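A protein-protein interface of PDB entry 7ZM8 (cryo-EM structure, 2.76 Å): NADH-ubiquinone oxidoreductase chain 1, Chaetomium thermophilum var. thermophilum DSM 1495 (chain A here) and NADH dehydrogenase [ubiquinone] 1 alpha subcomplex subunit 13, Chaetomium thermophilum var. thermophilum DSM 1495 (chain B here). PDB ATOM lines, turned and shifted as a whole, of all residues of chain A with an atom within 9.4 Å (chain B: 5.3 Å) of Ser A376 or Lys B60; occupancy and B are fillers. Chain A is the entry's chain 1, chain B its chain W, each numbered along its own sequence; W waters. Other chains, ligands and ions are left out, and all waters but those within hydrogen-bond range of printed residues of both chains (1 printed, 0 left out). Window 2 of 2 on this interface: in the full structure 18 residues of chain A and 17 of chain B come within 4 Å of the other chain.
Among the printed residues, merely in contact across the chains: Ser A376 with Lys B60 (3.3 Å), Leu A377 with Lys B60 (3.5 Å), Val A373 with Ala B57 (3.7 Å), Leu A377 with Ala B57 (3.7 Å), Ile A375 with Met B61 (3.9 Å) and Leu A377 with Leu B56 (3.9 Å).
Of the printed residues of chain B, Ile A375 touches Met B61. Printed residues of chain B within 4 Å of Ser A376: Lys B60 (3.3 Å). Printed residues of chain B within 4 Å of Leu A377: Leu B56, Ala B57 and Lys B60. Leu A378 touches none of the printed residues of chain B. Printed residues of chain A within 4 Å of Leu B56: Leu A377. Of the printed residues of chain A, Ala B57 touches Val A373 and Leu A377. Of chain A, only Ser A376 (3.3 Å) and Leu A377 (3.5 Å) come within 4 Å of Lys B60. Of chain A, only Ile A375 comes within 4 Å of Met B61. The nearest residue of chain B that does not touch Ser A376 is Arg B64 (4.7 Å). The nearest printed residue of chain A that does not touch Leu B56 is Leu A378 (4.8 Å).
Of the 10 printed residues of chain B, 4 touch a printed residue of chain A. Along chain B the printed residues that touch a printed residue of chain A span positions 56 to 61. Hydrophobic or aromatic side chains of chain A within 4 Å of the printed part of chain B: Val A373, Ile A375 and Leu A377. Among the printed residues, 6 pairs touch across the chains.
Water W1 lies within hydrogen-bond range of NH1 of Arg B64 (2.8 Å) and O of Ser A376 (2.8 Å).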
ATOM      1  N   ASP A 106     -14.977  11.136  31.060  1.00  0.00           N
ATOM      2  CA  ASP A 106     -14.560  10.712  29.700  1.00  0.00           C
ATOM      3  C   ASP A 106     -13.563  11.774  29.250  1.00  0.00           C
ATOM      4  O   ASP A 106     -14.003  12.774  28.677  1.00  0.00           O
ATOM      5  CB  ASP A 106     -15.778  10.534  28.799  1.00  0.00           C
ATOM      6  CG  ASP A 106     -15.491  10.216  27.341  1.00  0.00           C
ATOM      7  OD1 ASP A 106     -14.507   9.518  27.069  1.00  0.00           O
ATOM      8  OD2 ASP A 106     -16.265  10.670  26.488  1.00  0.00           O
ATOM      9  N   SER A 108     -10.251  13.261  27.135  1.00  0.00           N
ATOM     10  CA  SER A 108      -9.460  13.083  25.888  1.00  0.00           C
ATOM     11  C   SER A 108      -7.997  12.883  26.239  1.00  0.00           C
ATOM     12  O   SER A 108      -7.336  12.132  25.547  1.00  0.00           O
ATOM     13  CB  SER A 108      -9.650  14.249  24.980  1.00  0.00           C
ATOM     14  OG  SER A 108     -11.020  14.412  24.646  1.00  0.00           O
ATOM     15  N   GLY A 167      -3.788   6.884  18.045  1.00  0.00           N
ATOM     16  CA  GLY A 167      -3.957   8.267  17.674  1.00  0.00           C
ATOM     17  C   GLY A 167      -4.534   9.155  18.753  1.00  0.00           C
ATOM     18  O   GLY A 167      -4.533  10.379  18.589  1.00  0.00           O
ATOM     19  N   SER A 168      -5.007   8.588  19.858  1.00  0.00           N
ATOM     20  CA  SER A 168      -5.688   9.344  20.895  1.00  0.00           C
ATOM     21  C   SER A 168      -5.171   8.943  22.268  1.00  0.00           C
ATOM     22  O   SER A 168      -4.634   7.852  22.461  1.00  0.00           O
ATOM     23  CB  SER A 168      -7.203   9.129  20.836  1.00  0.00           C
ATOM     24  OG  SER A 168      -7.860   9.825  21.878  1.00  0.00           O
ATOM     25  N   SER A 170      -7.509   9.172  24.739  1.00  0.00           N
ATOM     26  CA  SER A 170      -8.786   8.799  25.403  1.00  0.00           C
ATOM     27  C   SER A 170      -8.844   7.283  25.538  1.00  0.00           C
ATOM     28  O   SER A 170      -8.793   6.615  24.515  1.00  0.00           O
ATOM     29  CB  SER A 170      -9.965   9.289  24.634  1.00  0.00           C
ATOM     30  OG  SER A 170     -11.158   8.665  25.070  1.00  0.00           O
ATOM     31  N   VAL A 173     -11.286   5.697  23.244  1.00  0.00           N
ATOM     32  CA  VAL A 173     -10.843   5.606  21.857  1.00  0.00           C
ATOM     33  C   VAL A 173      -9.777   4.532  21.704  1.00  0.00           C
ATOM     34  O   VAL A 173      -9.705   3.855  20.675  1.00  0.00           O
ATOM     35  CB  VAL A 173     -10.347   6.980  21.364  1.00  0.00           C
ATOM     36  CG1 VAL A 173      -9.938   6.914  19.902  1.00  0.00           C
ATOM     37  CG2 VAL A 173     -11.414   8.018  21.552  1.00  0.00           C
ATOM     38  N   VAL A 373      -6.156   9.001  12.023  1.00  0.00           N
ATOM     39  CA  VAL A 373      -6.573  10.426  12.106  1.00  0.00           C
ATOM     40  C   VAL A 373      -6.651  10.785  13.593  1.00  0.00           C
ATOM     41  O   VAL A 373      -6.882   9.875  14.411  1.00  0.00           O
ATOM     42  CB  VAL A 373      -7.904  10.647  11.368  1.00  0.00           C
ATOM     43  CG1 VAL A 373      -7.745  10.490   9.865  1.00  0.00           C
ATOM     44  CG2 VAL A 373      -8.993   9.722  11.889  1.00  0.00           C
ATOM     45  N   ASN A 374      -6.425  12.049  13.938  1.00  0.00           N
ATOM     46  CA  ASN A 374      -6.366  12.422  15.373  1.00  0.00           C
ATOM     47  C   ASN A 374      -7.610  13.244  15.706  1.00  0.00           C
ATOM     48  O   ASN A 374      -7.613  13.893  16.759  1.00  0.00           O
ATOM     49  CB  ASN A 374      -5.005  13.035  15.704  1.00  0.00           C
ATOM     50  CG  ASN A 374      -3.849  12.205  15.189  1.00  0.00           C
ATOM     51  OD1 ASN A 374      -3.201  12.575  14.216  1.00  0.00           O
ATOM     52  ND2 ASN A 374      -3.593  11.073  15.821  1.00  0.00           N
ATOM     53  N   ILE A 375      -8.606  13.231  14.823  1.00  0.00           N
ATOM     54  CA  ILE A 375      -9.906  13.916  15.080  1.00  0.00           C
ATOM     55  C   ILE A 375     -10.785  12.983  15.916  1.00  0.00           C
ATOM     56  O   ILE A 375     -10.421  11.807  16.063  1.00  0.00           O
ATOM     57  CB  ILE A 375     -10.583  14.324  13.755  1.00  0.00           C
ATOM     58  CG1 ILE A 375     -10.714  13.140  12.793  1.00  0.00           C
ATOM     59  CG2 ILE A 375      -9.830  15.476  13.119  1.00  0.00           C
ATOM     60  CD1 ILE A 375     -12.137  12.702  12.535  1.00  0.00           C
ATOM     61  N   SER A 376     -11.896  13.495  16.439  1.00  0.00           N
ATOM     62  CA  SER A 376     -12.843  12.651  17.206  1.00  0.00           C
ATOM     63  C   SER A 376     -13.624  11.721  16.281  1.00  0.00           C
ATOM     64  O   SER A 376     -14.564  12.200  15.638  1.00  0.00           O
ATOM     65  CB  SER A 376     -13.761  13.462  18.085  1.00  0.00           C
ATOM     66  OG  SER A 376     -13.021  14.197  19.048  1.00  0.00           O
ATOM     67  N   LEU A 377     -13.210  10.462  16.185  1.00  0.00           N
ATOM     68  CA  LEU A 377     -13.932   9.403  15.445  1.00  0.00           C
ATOM     69  C   LEU A 377     -13.884   8.261  16.450  1.00  0.00           C
ATOM     70  O   LEU A 377     -12.982   8.323  17.298  1.00  0.00           O
ATOM     71  CB  LEU A 377     -13.142   9.043  14.183  1.00  0.00           C
ATOM     72  CG  LEU A 377     -13.805   8.033  13.253  1.00  0.00           C
ATOM     73  CD1 LEU A 377     -14.706   8.737  12.252  1.00  0.00           C
ATOM     74  CD2 LEU A 377     -12.758   7.202  12.535  1.00  0.00           C
ATOM     75  N   LEU A 378     -14.796   7.297  16.407  1.00  0.00           N
ATOM     76  CA  LEU A 378     -14.655   6.166  17.363  1.00  0.00           C
ATOM     77  C   LEU A 378     -14.625   6.727  18.792  1.00  0.00           C
ATOM     78  O   LEU A 378     -14.075   6.041  19.674  1.00  0.00           O
ATOM     79  CB  LEU A 378     -13.377   5.375  17.049  1.00  0.00           C
ATOM     80  CG  LEU A 378     -13.551   4.104  16.225  1.00  0.00           C
ATOM     81  CD1 LEU A 378     -13.749   4.425  14.754  1.00  0.00           C
ATOM     82  CD2 LEU A 378     -12.337   3.216  16.396  1.00  0.00           C
ATOM     83  N   LEU B  56     -13.626   5.942   7.269  1.00  0.00           N
ATOM     84  CA  LEU B  56     -14.797   6.333   8.088  1.00  0.00           C
ATOM     85  C   LEU B  56     -14.682   7.806   8.446  1.00  0.00           C
ATOM     86  O   LEU B  56     -15.701   8.482   8.486  1.00  0.00           O
ATOM     87  CB  LEU B  56     -14.848   5.438   9.328  1.00  0.00           C
ATOM     88  CG  LEU B  56     -15.289   3.999   9.093  1.00  0.00           C
ATOM     89  CD1 LEU B  56     -15.150   3.197  10.372  1.00  0.00           C
ATOM     90  CD2 LEU B  56     -16.712   3.952   8.572  1.00  0.00           C
ATOM     91  N   ALA B  57     -13.471   8.267   8.715  1.00  0.00           N
ATOM     92  CA  ALA B  57     -13.212   9.685   9.018  1.00  0.00           C
ATOM     93  C   ALA B  57     -13.510  10.556   7.793  1.00  0.00           C
ATOM     94  O   ALA B  57     -14.013  11.667   7.983  1.00  0.00           O
ATOM     95  CB  ALA B  57     -11.813   9.854   9.547  1.00  0.00           C
ATOM     96  N   ARG B  58     -13.205  10.079   6.593  1.00  0.00           N
ATOM     97  CA  ARG B  58     -13.487  10.829   5.352  1.00  0.00           C
ATOM     98  C   ARG B  58     -14.993  11.023   5.215  1.00  0.00           C
ATOM     99  O   ARG B  58     -15.395  12.110   4.804  1.00  0.00           O
ATOM    100  CB  ARG B  58     -12.960  10.081   4.130  1.00  0.00           C
ATOM    101  CG  ARG B  58     -13.019  10.888   2.842  1.00  0.00           C
ATOM    102  CD  ARG B  58     -12.481  10.129   1.647  1.00  0.00           C
ATOM    103  NE  ARG B  58     -11.138   9.635   1.891  1.00  0.00           N
ATOM    104  CZ  ARG B  58     -10.030  10.321   1.653  1.00  0.00           C
ATOM    105  NH1 ARG B  58      -8.853   9.781   1.912  1.00  0.00           N
ATOM    106  NH2 ARG B  58     -10.099  11.541   1.160  1.00  0.00           N
ATOM    107  N   GLU B  59     -15.799  10.044   5.607  1.00  0.00           N
ATOM    108  CA  GLU B  59     -17.257  10.134   5.396  1.00  0.00           C
ATOM    109  C   GLU B  59     -17.844  11.008   6.496  1.00  0.00           C
ATOM    110  O   GLU B  59     -18.794  11.734   6.222  1.00  0.00           O
ATOM    111  CB  GLU B  59     -17.843   8.742   5.578  1.00  0.00           C
ATOM    112  CG  GLU B  59     -19.352   8.678   5.490  1.00  0.00           C
ATOM    113  CD  GLU B  59     -19.910   7.293   5.742  1.00  0.00           C
ATOM    114  OE1 GLU B  59     -19.146   6.434   6.212  1.00  0.00           O
ATOM    115  OE2 GLU B  59     -21.102   7.076   5.464  1.00  0.00           O
ATOM    116  N   LYS B  60     -17.256  10.972   7.680  1.00  0.00           N
ATOM    117  CA  LYS B  60     -17.700  11.850   8.778  1.00  0.00           C
ATOM    118  C   LYS B  60     -17.443  13.306   8.412  1.00  0.00           C
ATOM    119  O   LYS B  60     -18.303  14.141   8.714  1.00  0.00           O
ATOM    120  CB  LYS B  60     -16.961  11.484  10.059  1.00  0.00           C
ATOM    121  CG  LYS B  60     -17.548  12.082  11.327  1.00  0.00           C
ATOM    122  CD  LYS B  60     -16.596  12.082  12.487  1.00  0.00           C
ATOM    123  CE  LYS B  60     -17.280  11.718  13.783  1.00  0.00           C
ATOM    124  NZ  LYS B  60     -17.429  10.253  13.951  1.00  0.00           N
ATOM    125  N   MET B  61     -16.316  13.605   7.791  1.00  0.00           N
ATOM    126  CA  MET B  61     -15.966  15.009   7.490  1.00  0.00           C
ATOM    127  C   MET B  61     -16.909  15.532   6.417  1.00  0.00           C
ATOM    128  O   MET B  61     -17.438  16.613   6.603  1.00  0.00           O
ATOM    129  CB  MET B  61     -14.484  15.172   7.129  1.00  0.00           C
ATOM    130  CG  MET B  61     -13.547  14.980   8.312  1.00  0.00           C
ATOM    131  SD  MET B  61     -13.720  16.219   9.633  1.00  0.00           S
ATOM    132  CE  MET B  61     -14.540  15.261  10.906  1.00  0.00           C
ATOM    133  N   TRP B  62     -17.100  14.776   5.341  1.00  0.00           N
ATOM    134  CA  TRP B  62     -17.980  15.174   4.217  1.00  0.00           C
ATOM    135  C   TRP B  62     -19.410  15.339   4.708  1.00  0.00           C
ATOM    136  O   TRP B  62     -20.095  16.209   4.181  1.00  0.00           O
ATOM    137  CB  TRP B  62     -17.824  14.169   3.076  1.00  0.00           C
ATOM    138  CG  TRP B  62     -16.580  14.440   2.289  1.00  0.00           C
ATOM    139  CD1 TRP B  62     -15.441  13.691   2.252  1.00  0.00           C
ATOM    140  CD2 TRP B  62     -16.329  15.590   1.466  1.00  0.00           C
ATOM    141  NE1 TRP B  62     -14.511  14.280   1.441  1.00  0.00           N
ATOM    142  CE2 TRP B  62     -15.025  15.447   0.948  1.00  0.00           C
ATOM    143  CE3 TRP B  62     -17.082  16.709   1.101  1.00  0.00           C
ATOM    144  CZ2 TRP B  62     -14.461  16.388   0.091  1.00  0.00           C
ATOM    145  CZ3 TRP B  62     -16.525  17.636   0.255  1.00  0.00           C
ATOM    146  CH2 TRP B  62     -15.234  17.477  -0.242  1.00  0.00           C
ATOM    147  N   ALA B  63     -19.806  14.574   5.714  1.00  0.00           N
ATOM    148  CA  ALA B  63     -21.152  14.667   6.307  1.00  0.00           C
ATOM    149  C   ALA B  63     -21.311  16.004   7.045  1.00  0.00           C
ATOM    150  O   ALA B  63     -22.365  16.620   6.873  1.00  0.00           O
ATOM    151  CB  ALA B  63     -21.318  13.500   7.234  1.00  0.00           C
ATOM    152  N   ARG B  64     -20.302  16.441   7.800  1.00  0.00           N
ATOM    153  CA  ARG B  64     -20.300  17.741   8.512  1.00  0.00           C
ATOM    154  C   ARG B  64     -20.085  18.899   7.534  1.00  0.00           C
ATOM    155  O   ARG B  64     -20.660  19.949   7.787  1.00  0.00           O
ATOM    156  CB  ARG B  64     -19.293  17.729   9.662  1.00  0.00           C
ATOM    157  CG  ARG B  64     -19.556  16.722  10.765  1.00  0.00           C
ATOM    158  CD  ARG B  64     -18.415  16.950  11.727  1.00  0.00           C
ATOM    159  NE  ARG B  64     -18.530  16.134  12.916  1.00  0.00           N
ATOM    160  CZ  ARG B  64     -17.693  16.179  13.930  1.00  0.00           C
ATOM    161  NH1 ARG B  64     -17.890  15.409  14.981  1.00  0.00           N
ATOM    162  NH2 ARG B  64     -16.674  17.011  13.905  1.00  0.00           N
ATOM    163  N   ILE B  65     -19.348  18.713   6.437  1.00  0.00           N
ATOM    164  CA  ILE B  65     -19.181  19.767   5.394  1.00  0.00           C
ATOM    165  C   ILE B  65     -20.519  20.105   4.723  1.00  0.00           C
ATOM    166  O   ILE B  65     -20.802  21.298   4.567  1.00  0.00           O
ATOM    167  CB  ILE B  65     -18.092  19.376   4.380  1.00  0.00           C
ATOM    168  CG1 ILE B  65     -16.687  19.554   4.956  1.00  0.00           C
ATOM    169  CG2 ILE B  65     -18.269  20.106   3.056  1.00  0.00           C
ATOM    170  CD1 ILE B  65     -15.663  18.637   4.336  1.00  0.00           C
HETATM  171  O   HOH W   1     -17.009  13.241  16.458  1.00  0.00           O
